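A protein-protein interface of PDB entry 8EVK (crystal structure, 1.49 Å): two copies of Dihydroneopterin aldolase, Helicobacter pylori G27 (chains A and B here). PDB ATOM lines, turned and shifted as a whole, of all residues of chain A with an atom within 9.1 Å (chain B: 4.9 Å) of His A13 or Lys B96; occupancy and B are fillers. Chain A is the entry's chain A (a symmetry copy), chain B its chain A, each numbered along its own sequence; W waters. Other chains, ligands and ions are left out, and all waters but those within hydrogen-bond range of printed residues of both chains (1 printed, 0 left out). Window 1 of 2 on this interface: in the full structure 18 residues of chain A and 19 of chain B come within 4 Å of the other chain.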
ATOM      1  N   GLY A   9      14.381 -10.359  22.771  1.00  0.00           N
ATOM      2  CA  GLY A   9      15.312 -11.339  22.251  1.00  0.00           C
ATOM      3  C   GLY A   9      15.593 -12.438  23.254  1.00  0.00           C
ATOM      4  O   GLY A   9      15.575 -12.228  24.471  1.00  0.00           O
ATOM      5  N   VAL A  10      15.827 -13.636  22.720  1.00  0.00           N
ATOM      6  CA  VAL A  10      16.419 -14.736  23.462  1.00  0.00           C
ATOM      7  C   VAL A  10      17.754 -15.054  22.804  1.00  0.00           C
ATOM      8  O   VAL A  10      17.861 -15.079  21.569  1.00  0.00           O
ATOM      9  CB  VAL A  10      15.488 -15.963  23.497  1.00  0.00           C
ATOM     10  CG1 VAL A  10      16.174 -17.121  24.176  1.00  0.00           C
ATOM     11  CG2 VAL A  10      14.199 -15.611  24.224  1.00  0.00           C
ATOM     12  N   HIS A  11      18.777 -15.272  23.624  1.00  0.00           N
ATOM     13  CA  HIS A  11      20.148 -15.360  23.131  1.00  0.00           C
ATOM     14  C   HIS A  11      20.820 -16.606  23.675  1.00  0.00           C
ATOM     15  O   HIS A  11      20.774 -16.862  24.881  1.00  0.00           O
ATOM     16  CB  HIS A  11      20.937 -14.108  23.524  1.00  0.00           C
ATOM     17  CG  HIS A  11      20.229 -12.839  23.177  1.00  0.00           C
ATOM     18  ND1 HIS A  11      20.230 -12.324  21.897  1.00  0.00           N
ATOM     19  CD2 HIS A  11      19.504 -11.977  23.931  1.00  0.00           C
ATOM     20  CE1 HIS A  11      19.524 -11.203  21.877  1.00  0.00           C
ATOM     21  NE2 HIS A  11      19.077 -10.969  23.099  1.00  0.00           N
ATOM     22  N   VAL A  12      21.407 -17.396  22.777  1.00  0.00           N
ATOM     23  CA  VAL A  12      22.289 -18.495  23.140  1.00  0.00           C
ATOM     24  C   VAL A  12      23.610 -18.203  22.463  1.00  0.00           C
ATOM     25  O   VAL A  12      23.718 -18.319  21.239  1.00  0.00           O
ATOM     26  CB  VAL A  12      21.734 -19.848  22.687  1.00  0.00           C
ATOM     27  CG1 VAL A  12      22.775 -20.946  22.981  1.00  0.00           C
ATOM     28  CG2 VAL A  12      20.397 -20.154  23.344  1.00  0.00           C
ATOM     29  N   HIS A  13      24.633 -17.857  23.240  1.00  0.00           N
ATOM     30  CA  HIS A  13      25.894 -17.436  22.660  1.00  0.00           C
ATOM     31  C   HIS A  13      27.001 -18.379  23.101  1.00  0.00           C
ATOM     32  O   HIS A  13      26.941 -18.950  24.196  1.00  0.00           O
ATOM     33  CB  HIS A  13      26.245 -15.997  23.047  1.00  0.00           C
ATOM     34  CG  HIS A  13      25.441 -14.968  22.313  1.00  0.00           C
ATOM     35  ND1 HIS A  13      25.665 -13.613  22.436  1.00  0.00           N
ATOM     36  CD2 HIS A  13      24.393 -15.102  21.461  1.00  0.00           C
ATOM     37  CE1 HIS A  13      24.802 -12.954  21.680  1.00  0.00           C
ATOM     38  NE2 HIS A  13      24.017 -13.833  21.079  1.00  0.00           N
ATOM     39  N   ASN A  14      27.979 -18.555  22.214  1.00  0.00           N
ATOM     40  CA  ASN A  14      29.158 -19.389  22.482  1.00  0.00           C
ATOM     41  C   ASN A  14      28.767 -20.793  22.920  1.00  0.00           C
ATOM     42  O   ASN A  14      29.375 -21.383  23.818  1.00  0.00           O
ATOM     43  CB  ASN A  14      30.096 -18.729  23.493  1.00  0.00           C
ATOM     44  CG  ASN A  14      30.500 -17.340  23.073  1.00  0.00           C
ATOM     45  OD1 ASN A  14      30.947 -17.126  21.946  1.00  0.00           O
ATOM     46  ND2 ASN A  14      30.332 -16.375  23.972  1.00  0.00           N
ATOM     47  N   LEU A  15      27.707 -21.319  22.316  1.00  0.00           N
ATOM     48  CA  LEU A  15      27.320 -22.707  22.535  1.00  0.00           C
ATOM     49  C   LEU A  15      28.360 -23.590  21.860  1.00  0.00           C
ATOM     50  O   LEU A  15      28.492 -23.582  20.632  1.00  0.00           O
ATOM     51  CB  LEU A  15      25.937 -22.955  21.936  1.00  0.00           C
ATOM     52  CG  LEU A  15      25.458 -24.411  21.852  1.00  0.00           C
ATOM     53  CD1 LEU A  15      25.460 -25.102  23.225  1.00  0.00           C
ATOM     54  CD2 LEU A  15      24.084 -24.526  21.166  1.00  0.00           C
ATOM     55  N   VAL A  16      29.125 -24.337  22.653  1.00  0.00           N
ATOM     56  CA  VAL A  16      30.273 -25.078  22.147  1.00  0.00           C
ATOM     57  C   VAL A  16      30.020 -26.564  22.345  1.00  0.00           C
ATOM     58  O   VAL A  16      29.606 -26.995  23.428  1.00  0.00           O
ATOM     59  CB  VAL A  16      31.588 -24.632  22.814  1.00  0.00           C
ATOM     60  CG1 VAL A  16      32.741 -25.462  22.295  1.00  0.00           C
ATOM     61  CG2 VAL A  16      31.855 -23.168  22.530  1.00  0.00           C
ATOM     62  N   ILE A  34      32.860 -26.778  17.504  1.00  0.00           N
ATOM     63  CA  ILE A  34      32.232 -25.620  16.896  1.00  0.00           C
ATOM     64  C   ILE A  34      31.643 -24.734  17.987  1.00  0.00           C
ATOM     65  O   ILE A  34      31.471 -25.143  19.133  1.00  0.00           O
ATOM     66  CB  ILE A  34      31.171 -25.996  15.850  1.00  0.00           C
ATOM     67  CG1 ILE A  34      29.968 -26.642  16.526  1.00  0.00           C
ATOM     68  CG2 ILE A  34      31.761 -26.931  14.807  1.00  0.00           C
ATOM     69  CD1 ILE A  34      28.750 -26.643  15.650  1.00  0.00           C
ATOM     70  N   SER A  35      31.292 -23.514  17.592  1.00  0.00           N
ATOM     71  CA  SER A  35      30.690 -22.554  18.500  1.00  0.00           C
ATOM     72  C   SER A  35      29.521 -21.932  17.755  1.00  0.00           C
ATOM     73  O   SER A  35      29.687 -21.498  16.613  1.00  0.00           O
ATOM     74  CB  SER A  35      31.713 -21.473  18.844  1.00  0.00           C
ATOM     75  OG  SER A  35      31.199 -20.536  19.778  1.00  0.00           O
ATOM     76  N   VAL A  36      28.353 -21.905  18.391  1.00  0.00           N
ATOM     77  CA  VAL A  36      27.129 -21.409  17.753  1.00  0.00           C
ATOM     78  C   VAL A  36      26.623 -20.198  18.522  1.00  0.00           C
ATOM     79  O   VAL A  36      26.565 -20.213  19.757  1.00  0.00           O
ATOM     80  CB  VAL A  36      26.044 -22.498  17.741  1.00  0.00           C
ATOM     81  CG1 VAL A  36      24.825 -22.033  16.957  1.00  0.00           C
ATOM     82  CG2 VAL A  36      26.580 -23.789  17.143  1.00  0.00           C
ATOM     83  N   ASP A  37      26.209 -19.160  17.792  1.00  0.00           N
ATOM     84  CA  ASP A  37      25.520 -18.021  18.387  1.00  0.00           C
ATOM     85  C   ASP A  37      24.147 -17.935  17.743  1.00  0.00           C
ATOM     86  O   ASP A  37      24.033 -17.999  16.510  1.00  0.00           O
ATOM     87  CB  ASP A  37      26.244 -16.716  18.086  1.00  0.00           C
ATOM     88  CG  ASP A  37      27.629 -16.648  18.717  1.00  0.00           C
ATOM     89  OD1 ASP A  37      27.826 -17.239  19.803  1.00  0.00           O
ATOM     90  OD2 ASP A  37      28.516 -15.994  18.118  1.00  0.00           O
ATOM     91  N   LEU A  38      23.114 -17.822  18.563  1.00  0.00           N
ATOM     92  CA  LEU A  38      21.748 -17.682  18.069  1.00  0.00           C
ATOM     93  C   LEU A  38      21.045 -16.541  18.787  1.00  0.00           C
ATOM     94  O   LEU A  38      21.050 -16.482  20.021  1.00  0.00           O
ATOM     95  CB  LEU A  38      20.973 -18.975  18.260  1.00  0.00           C
ATOM     96  CG  LEU A  38      19.514 -18.852  17.855  1.00  0.00           C
ATOM     97  CD1 LEU A  38      19.350 -18.684  16.339  1.00  0.00           C
ATOM     98  CD2 LEU A  38      18.808 -20.093  18.330  1.00  0.00           C
ATOM     99  N   ASP A  39      20.425 -15.652  18.017  1.00  0.00           N
ATOM    100  CA  ASP A  39      19.531 -14.634  18.548  1.00  0.00           C
ATOM    101  C   ASP A  39      18.177 -14.857  17.900  1.00  0.00           C
ATOM    102  O   ASP A  39      18.090 -14.980  16.671  1.00  0.00           O
ATOM    103  CB  ASP A  39      19.967 -13.206  18.201  1.00  0.00           C
ATOM    104  CG  ASP A  39      21.361 -12.885  18.656  1.00  0.00           C
ATOM    105  OD1 ASP A  39      21.710 -13.228  19.801  1.00  0.00           O
ATOM    106  OD2 ASP A  39      22.126 -12.316  17.848  1.00  0.00           O
ATOM    107  N   LEU A  40      17.132 -14.920  18.712  1.00  0.00           N
ATOM    108  CA  LEU A  40      15.765 -14.991  18.213  1.00  0.00           C
ATOM    109  C   LEU A  40      15.035 -13.766  18.731  1.00  0.00           C
ATOM    110  O   LEU A  40      15.027 -13.524  19.942  1.00  0.00           O
ATOM    111  CB  LEU A  40      15.060 -16.239  18.736  1.00  0.00           C
ATOM    112  CG  LEU A  40      15.601 -17.588  18.235  1.00  0.00           C
ATOM    113  CD1 LEU A  40      14.852 -18.750  18.885  1.00  0.00           C
ATOM    114  CD2 LEU A  40      15.506 -17.680  16.722  1.00  0.00           C
ATOM    115  N   PHE A  41      14.405 -13.015  17.839  1.00  0.00           N
ATOM    116  CA  PHE A  41      13.732 -11.784  18.234  1.00  0.00           C
ATOM    117  C   PHE A  41      12.243 -11.895  17.941  1.00  0.00           C
ATOM    118  O   PHE A  41      11.833 -12.566  16.988  1.00  0.00           O
ATOM    119  CB  PHE A  41      14.299 -10.579  17.501  1.00  0.00           C
ATOM    120  CG  PHE A  41      15.744 -10.302  17.809  1.00  0.00           C
ATOM    121  CD1 PHE A  41      16.113  -9.681  18.995  1.00  0.00           C
ATOM    122  CD2 PHE A  41      16.727 -10.662  16.909  1.00  0.00           C
ATOM    123  CE1 PHE A  41      17.454  -9.413  19.273  1.00  0.00           C
ATOM    124  CE2 PHE A  41      18.067 -10.397  17.175  1.00  0.00           C
ATOM    125  CZ  PHE A  41      18.431  -9.780  18.358  1.00  0.00           C
ATOM    126  N   TYR A  53      15.194 -21.211  26.249  1.00  0.00           N
ATOM    127  CA  TYR A  53      16.573 -21.387  25.814  1.00  0.00           C
ATOM    128  C   TYR A  53      17.073 -22.813  26.019  1.00  0.00           C
ATOM    129  O   TYR A  53      18.014 -23.228  25.336  1.00  0.00           O
ATOM    130  CB  TYR A  53      17.516 -20.349  26.447  1.00  0.00           C
ATOM    131  CG  TYR A  53      17.541 -20.306  27.962  1.00  0.00           C
ATOM    132  CD1 TYR A  53      18.071 -21.358  28.698  1.00  0.00           C
ATOM    133  CD2 TYR A  53      17.049 -19.203  28.652  1.00  0.00           C
ATOM    134  CE1 TYR A  53      18.103 -21.329  30.081  1.00  0.00           C
ATOM    135  CE2 TYR A  53      17.084 -19.155  30.042  1.00  0.00           C
ATOM    136  CZ  TYR A  53      17.605 -20.234  30.749  1.00  0.00           C
ATOM    137  OH  TYR A  53      17.644 -20.221  32.122  1.00  0.00           O
ATOM    138  N   ILE A  56      15.975 -24.713  22.980  1.00  0.00           N
ATOM    139  CA  ILE A  56      16.625 -24.151  21.801  1.00  0.00           C
ATOM    140  C   ILE A  56      18.036 -24.699  21.672  1.00  0.00           C
ATOM    141  O   ILE A  56      18.462 -25.153  20.597  1.00  0.00           O
ATOM    142  CB  ILE A  56      16.608 -22.614  21.880  1.00  0.00           C
ATOM    143  CG1 ILE A  56      15.202 -22.077  21.619  1.00  0.00           C
ATOM    144  CG2 ILE A  56      17.581 -22.033  20.876  1.00  0.00           C
ATOM    145  CD1 ILE A  56      15.021 -20.635  22.040  1.00  0.00           C
ATOM    146  N   GLN A  57      18.776 -24.684  22.775  1.00  0.00           N
ATOM    147  CA  GLN A  57      20.133 -25.200  22.786  1.00  0.00           C
ATOM    148  C   GLN A  57      20.150 -26.688  22.470  1.00  0.00           C
ATOM    149  O   GLN A  57      20.973 -27.154  21.676  1.00  0.00           O
ATOM    150  CB  GLN A  57      20.733 -24.910  24.162  1.00  0.00           C
ATOM    151  CG  GLN A  57      22.136 -25.359  24.373  1.00  0.00           C
ATOM    152  CD  GLN A  57      22.747 -24.673  25.576  1.00  0.00           C
ATOM    153  OE1 GLN A  57      22.463 -23.502  25.835  1.00  0.00           O
ATOM    154  NE2 GLN A  57      23.590 -25.388  26.312  1.00  0.00           N
ATOM    155  N   ILE A  60      19.517 -27.351  18.681  1.00  0.00           N
ATOM    156  CA  ILE A  60      20.661 -27.042  17.824  1.00  0.00           C
ATOM    157  C   ILE A  60      21.690 -28.157  17.886  1.00  0.00           C
ATOM    158  O   ILE A  60      22.181 -28.632  16.855  1.00  0.00           O
ATOM    159  CB  ILE A  60      21.286 -25.697  18.220  1.00  0.00           C
ATOM    160  CG1 ILE A  60      20.359 -24.554  17.828  1.00  0.00           C
ATOM    161  CG2 ILE A  60      22.649 -25.535  17.532  1.00  0.00           C
ATOM    162  CD1 ILE A  60      20.730 -23.252  18.488  1.00  0.00           C
ATOM    163  N   TYR A  94      19.031 -14.548  13.940  1.00  0.00           N
ATOM    164  CA  TYR A  94      20.431 -14.453  13.562  1.00  0.00           C
ATOM    165  C   TYR A  94      21.122 -15.702  14.072  1.00  0.00           C
ATOM    166  O   TYR A  94      21.007 -16.024  15.256  1.00  0.00           O
ATOM    167  CB  TYR A  94      21.111 -13.221  14.166  1.00  0.00           C
ATOM    168  CG  TYR A  94      22.589 -13.170  13.847  1.00  0.00           C
ATOM    169  CD1 TYR A  94      23.015 -12.921  12.560  1.00  0.00           C
ATOM    170  CD2 TYR A  94      23.557 -13.410  14.819  1.00  0.00           C
ATOM    171  CE1 TYR A  94      24.346 -12.873  12.231  1.00  0.00           C
ATOM    172  CE2 TYR A  94      24.917 -13.362  14.494  1.00  0.00           C
ATOM    173  CZ  TYR A  94      25.287 -13.086  13.190  1.00  0.00           C
ATOM    174  OH  TYR A  94      26.603 -13.037  12.806  1.00  0.00           O
ATOM    175  N   LEU A  95      21.793 -16.424  13.183  1.00  0.00           N
ATOM    176  CA  LEU A  95      22.475 -17.655  13.551  1.00  0.00           C
ATOM    177  C   LEU A  95      23.847 -17.659  12.912  1.00  0.00           C
ATOM    178  O   LEU A  95      23.965 -17.463  11.700  1.00  0.00           O
ATOM    179  CB  LEU A  95      21.661 -18.868  13.062  1.00  0.00           C
ATOM    180  CG  LEU A  95      22.236 -20.265  13.214  1.00  0.00           C
ATOM    181  CD1 LEU A  95      22.365 -20.660  14.664  1.00  0.00           C
ATOM    182  CD2 LEU A  95      21.313 -21.255  12.469  1.00  0.00           C
ATOM    183  N   LYS A  96      24.880 -17.890  13.721  1.00  0.00           N
ATOM    184  CA  LYS A  96      26.244 -17.938  13.213  1.00  0.00           C
ATOM    185  C   LYS A  96      26.891 -19.202  13.747  1.00  0.00           C
ATOM    186  O   LYS A  96      26.767 -19.514  14.939  1.00  0.00           O
ATOM    187  CB  LYS A  96      27.051 -16.708  13.659  1.00  0.00           C
ATOM    188  CG  LYS A  96      28.467 -16.672  13.064  1.00  0.00           C
ATOM    189  CD  LYS A  96      29.212 -15.417  13.499  1.00  0.00           C
ATOM    190  CE  LYS A  96      30.676 -15.531  13.111  1.00  0.00           C
ATOM    191  NZ  LYS A  96      31.443 -14.324  13.533  1.00  0.00           N
ATOM    192  N   SER B  35      24.720 -11.572  34.845  1.00  0.00           N
ATOM    193  CA  SER B  35      25.460 -10.460  34.275  1.00  0.00           C
ATOM    194  C   SER B  35      24.450  -9.617  33.515  1.00  0.00           C
ATOM    195  O   SER B  35      23.678 -10.157  32.721  1.00  0.00           O
ATOM    196  CB  SER B  35      26.512 -10.996  33.307  1.00  0.00           C
ATOM    197  OG  SER B  35      27.309  -9.954  32.763  1.00  0.00           O
ATOM    198  N   VAL B  36      24.449  -8.311  33.771  1.00  0.00           N
ATOM    199  CA  VAL B  36      23.471  -7.399  33.169  1.00  0.00           C
ATOM    200  C   VAL B  36      24.205  -6.378  32.311  1.00  0.00           C
ATOM    201  O   VAL B  36      25.217  -5.808  32.735  1.00  0.00           O
ATOM    202  CB  VAL B  36      22.667  -6.670  34.257  1.00  0.00           C
ATOM    203  CG1 VAL B  36      21.560  -5.830  33.636  1.00  0.00           C
ATOM    204  CG2 VAL B  36      22.072  -7.660  35.245  1.00  0.00           C
ATOM    205  N   ASP B  37      23.670  -6.110  31.118  1.00  0.00           N
ATOM    206  CA  ASP B  37      24.152  -5.016  30.282  1.00  0.00           C
ATOM    207  C   ASP B  37      22.991  -4.059  30.073  1.00  0.00           C
ATOM    208  O   ASP B  37      21.879  -4.493  29.735  1.00  0.00           O
ATOM    209  CB  ASP B  37      24.581  -5.515  28.909  1.00  0.00           C
ATOM    210  CG  ASP B  37      25.777  -6.456  28.968  1.00  0.00           C
ATOM    211  OD1 ASP B  37      26.629  -6.292  29.870  1.00  0.00           O
ATOM    212  OD2 ASP B  37      25.858  -7.359  28.100  1.00  0.00           O
ATOM    213  N   LEU B  76      12.956  -8.258  32.730  1.00  0.00           N
ATOM    214  CA  LEU B  76      13.150  -7.245  31.692  1.00  0.00           C
ATOM    215  C   LEU B  76      11.946  -6.323  31.594  1.00  0.00           C
ATOM    216  O   LEU B  76      12.091  -5.113  31.374  1.00  0.00           O
ATOM    217  CB  LEU B  76      13.354  -7.927  30.352  1.00  0.00           C
ATOM    218  CG  LEU B  76      14.642  -8.714  30.191  1.00  0.00           C
ATOM    219  CD1 LEU B  76      14.568  -9.457  28.855  1.00  0.00           C
ATOM    220  CD2 LEU B  76      15.856  -7.814  30.264  1.00  0.00           C
ATOM    221  N   TYR B  94      18.290  -0.459  25.944  1.00  0.00           N
ATOM    222  CA  TYR B  94      18.648  -1.836  25.645  1.00  0.00           C
ATOM    223  C   TYR B  94      19.072  -2.485  26.947  1.00  0.00           C
ATOM    224  O   TYR B  94      19.932  -1.949  27.646  1.00  0.00           O
ATOM    225  CB  TYR B  94      19.802  -1.927  24.640  1.00  0.00           C
ATOM    226  CG  TYR B  94      20.235  -3.357  24.397  1.00  0.00           C
ATOM    227  CD1 TYR B  94      19.413  -4.226  23.713  1.00  0.00           C
ATOM    228  CD2 TYR B  94      21.443  -3.849  24.883  1.00  0.00           C
ATOM    229  CE1 TYR B  94      19.769  -5.530  23.479  1.00  0.00           C
ATOM    230  CE2 TYR B  94      21.816  -5.177  24.648  1.00  0.00           C
ATOM    231  CZ  TYR B  94      20.961  -5.999  23.937  1.00  0.00           C
ATOM    232  OH  TYR B  94      21.263  -7.312  23.684  1.00  0.00           O
ATOM    233  N   LEU B  95      18.443  -3.602  27.294  1.00  0.00           N
ATOM    234  CA  LEU B  95      18.746  -4.300  28.534  1.00  0.00           C
ATOM    235  C   LEU B  95      18.845  -5.782  28.243  1.00  0.00           C
ATOM    236  O   LEU B  95      17.929  -6.360  27.652  1.00  0.00           O
ATOM    237  CB  LEU B  95      17.633  -4.037  29.566  1.00  0.00           C
ATOM    238  CG  LEU B  95      17.660  -4.767  30.897  1.00  0.00           C
ATOM    239  CD1 LEU B  95      18.841  -4.348  31.738  1.00  0.00           C
ATOM    240  CD2 LEU B  95      16.340  -4.470  31.641  1.00  0.00           C
ATOM    241  N   LYS B  96      19.949  -6.399  28.664  1.00  0.00           N
ATOM    242  CA  LYS B  96      20.143  -7.828  28.459  1.00  0.00           C
ATOM    243  C   LYS B  96      20.562  -8.432  29.786  1.00  0.00           C
ATOM    244  O   LYS B  96      21.428  -7.882  30.479  1.00  0.00           O
ATOM    245  CB  LYS B  96      21.221  -8.099  27.397  1.00  0.00           C
ATOM    246  CG  LYS B  96      21.389  -9.593  27.080  1.00  0.00           C
ATOM    247  CD  LYS B  96      22.435  -9.810  25.995  1.00  0.00           C
ATOM    248  CE  LYS B  96      22.760 -11.289  25.885  1.00  0.00           C
ATOM    249  NZ  LYS B  96      23.793 -11.540  24.839  1.00  0.00           N
ATOM    250  N   ILE B  97      19.926  -9.536  30.152  1.00  0.00           N
ATOM    251  CA  ILE B  97      20.245 -10.249  31.383  1.00  0.00           C
ATOM    252  C   ILE B  97      20.699 -11.663  31.028  1.00  0.00           C
ATOM    253  O   ILE B  97      19.987 -12.387  30.326  1.00  0.00           O
ATOM    254  CB  ILE B  97      19.037 -10.269  32.335  1.00  0.00           C
ATOM    255  CG1 ILE B  97      18.722  -8.822  32.792  1.00  0.00           C
ATOM    256  CG2 ILE B  97      19.311 -11.210  33.503  1.00  0.00           C
ATOM    257  CD1 ILE B  97      17.318  -8.634  33.462  1.00  0.00           C
ATOM    258  N   SER B  98      21.884 -12.047  31.492  1.00  0.00           N
ATOM    259  CA  SER B  98      22.432 -13.355  31.169  1.00  0.00           C
ATOM    260  C   SER B  98      22.676 -14.143  32.437  1.00  0.00           C
ATOM    261  O   SER B  98      23.070 -13.578  33.465  1.00  0.00           O
ATOM    262  CB  SER B  98      23.732 -13.296  30.349  1.00  0.00           C
ATOM    263  OG  SER B  98      23.679 -12.350  29.301  1.00  0.00           O
ATOM    264  N   SER B 106      27.509 -22.849  27.346  1.00  0.00           N
ATOM    265  CA  SER B 106      27.016 -21.701  26.597  1.00  0.00           C
ATOM    266  C   SER B 106      26.729 -20.562  27.563  1.00  0.00           C
ATOM    267  O   SER B 106      26.755 -20.727  28.784  1.00  0.00           O
ATOM    268  CB  SER B 106      25.727 -22.053  25.858  1.00  0.00           C
ATOM    269  OG  SER B 106      24.719 -22.430  26.784  1.00  0.00           O
ATOM    270  N   GLN B 107      26.418 -19.407  26.992  1.00  0.00           N
ATOM    271  CA  GLN B 107      25.916 -18.269  27.745  1.00  0.00           C
ATOM    272  C   GLN B 107      24.526 -17.976  27.210  1.00  0.00           C
ATOM    273  O   GLN B 107      24.366 -17.760  26.006  1.00  0.00           O
ATOM    274  CB  GLN B 107      26.837 -17.063  27.556  1.00  0.00           C
ATOM    275  CG  GLN B 107      28.290 -17.361  27.907  1.00  0.00           C
ATOM    276  CD  GLN B 107      29.284 -16.630  27.019  1.00  0.00           C
ATOM    277  OE1 GLN B 107      28.945 -15.639  26.368  1.00  0.00           O
ATOM    278  NE2 GLN B 107      30.524 -17.120  26.989  1.00  0.00           N
ATOM    279  N   GLY B 109      20.696 -15.882  27.673  1.00  0.00           N
ATOM    280  CA  GLY B 109      20.146 -14.653  28.212  1.00  0.00           C
ATOM    281  C   GLY B 109      18.939 -14.222  27.414  1.00  0.00           C
ATOM    282  O   GLY B 109      18.527 -14.872  26.452  1.00  0.00           O
ATOM    283  N   ALA B 110      18.348 -13.116  27.857  1.00  0.00           N
ATOM    284  CA  ALA B 110      17.227 -12.514  27.165  1.00  0.00           C
ATOM    285  C   ALA B 110      17.412 -11.010  27.236  1.00  0.00           C
ATOM    286  O   ALA B 110      18.046 -10.491  28.158  1.00  0.00           O
ATOM    287  CB  ALA B 110      15.863 -12.928  27.757  1.00  0.00           C
ATOM    288  N   SER B 111      16.874 -10.318  26.241  1.00  0.00           N
ATOM    289  CA  SER B 111      17.031  -8.878  26.156  1.00  0.00           C
ATOM    290  C   SER B 111      15.741  -8.215  25.723  1.00  0.00           C
ATOM    291  O   SER B 111      14.809  -8.844  25.217  1.00  0.00           O
ATOM    292  CB  SER B 111      18.105  -8.500  25.155  1.00  0.00           C
ATOM    293  OG  SER B 111      17.716  -8.891  23.841  1.00  0.00           O
HETATM  294  O   HOH W   1      26.907 -12.910  25.179  1.00  0.00           O
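Positions printed for both chains: 35, 36, 37, 94, 95 and 96. Of the 16 pairs that touch across the chains among the printed residues, none has its exchanged pair printed and touching as well.
The backbone carbonyl oxygen of Asp B37 is in hydrogen-bond range of the backbone NH of Lys B96 (2.9 Å). The backbone NH (N) of Ile B97 lies within hydrogen-bond range of the backbone carbonyl oxygen (O) of Ala B110 (2.9 Å). The side-chain carboxylate of Asp A39 lies within hydrogen-bond range of a ring nitrogen (ND1) of His A11 (2.7 Å). The backbone NH (N) of Leu A38 sits at hydrogen-bond distance from the backbone carbonyl oxygen (O) of Val A12 (2.8 Å). A ring nitrogen (NE2) of His A13 lies within hydrogen-bond range of the side-chain carboxylate of Asp A39, at 2.7 Å. The backbone carbonyl oxygen (O) of Val A36 is in hydrogen-bond range of the backbone NH (N) of Asn A14, 3.3 Å away.
OG of Ser B106 sits at hydrogen-bond distance from OE1 of Gln A57 (2.7 Å). The backbone NH (N) of His A13 sits at hydrogen-bond distance from the backbone carbonyl oxygen (O) of Gln B107, at 2.8 Å. OE1 of Gln B107 sits at hydrogen-bond distance from ND2 of Asn A14. The backbone carbonyl oxygen of Gly B109 is in hydrogen-bond range of the backbone NH of His A11, 2.9 Å away. The backbone carbonyl oxygen of Ser B111 sits at hydrogen-bond distance from the backbone NH of Gly A9, at 2.9 Å. NE2 of His A11 lies within hydrogen-bond range of OG of Ser B111, 2.6 Å away.
Of the 14 printed residues of chain B, 6 touch a printed residue of chain A. Printed residues of chain B that touch a printed residue of chain A: Lys B96, Ser B106, Gln B107, Gly B109, Ala B110 and Ser B111. Hydrophobic or aromatic side chains of chain B within 4 Å of the printed part of chain A: Ala B110. Of the 23 printed residues of chain A, 8 touch a printed residue of chain B. Hydrophobic or aromatic side chains of chain A within 4 Å of the printed part of chain B: Val A10, His A11 and His A13. Along chain A the printed residues that touch a printed residue of chain B span positions 9 to 57. Among the printed residues, 16 pairs touch across the chains.
Water W1 bridges ND1 of His A13 (3.1 Å) and NZ of Lys B96 (3.4 Å).
Printed residues of chain B within 4 Å of Val A12: Gln B107. His A13 touches just these residues of chain B: Lys B96, Ser B106 and Gln B107. No residue of chain A comes within 4 Å of Val B36. Lys B96 touches two residues of chain A. Ser B106 touches just these residues of chain A: His A13 (3.7 Å), Asn A14 (3.7 Å), Leu A15 (3.7 Å) and Gln A57 (2.7 Å). Of the printed residues of chain A, Gln B107 touches His A11, Val A12, His A13 and Asn A14. Of the printed residues of chain A, Ala B110 touches Gly A9 and His A11. Of the printed residues of chain A, Ser B111 touches Gly A9 and His A11.
Among the printed residues, pairs that only touch across the chains: Gly A9 with Ala B110 (3.2 Å), His A13 with Lys B96 (3.6 Å), Val A12 with Gln B107 (3.6 Å), His A13 with Ser B106 (3.7 Å), Asn A14 with Ser B106 (3.7 Å), Val A10 with Gly B109 (3.7 Å), Leu A15 with Ser B106 (3.7 Å), His A11 with Lys B96 (3.9 Å), His A11 with Gln B107 (3.9 Å) and His A11 with Ala B110 (3.99 Å).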
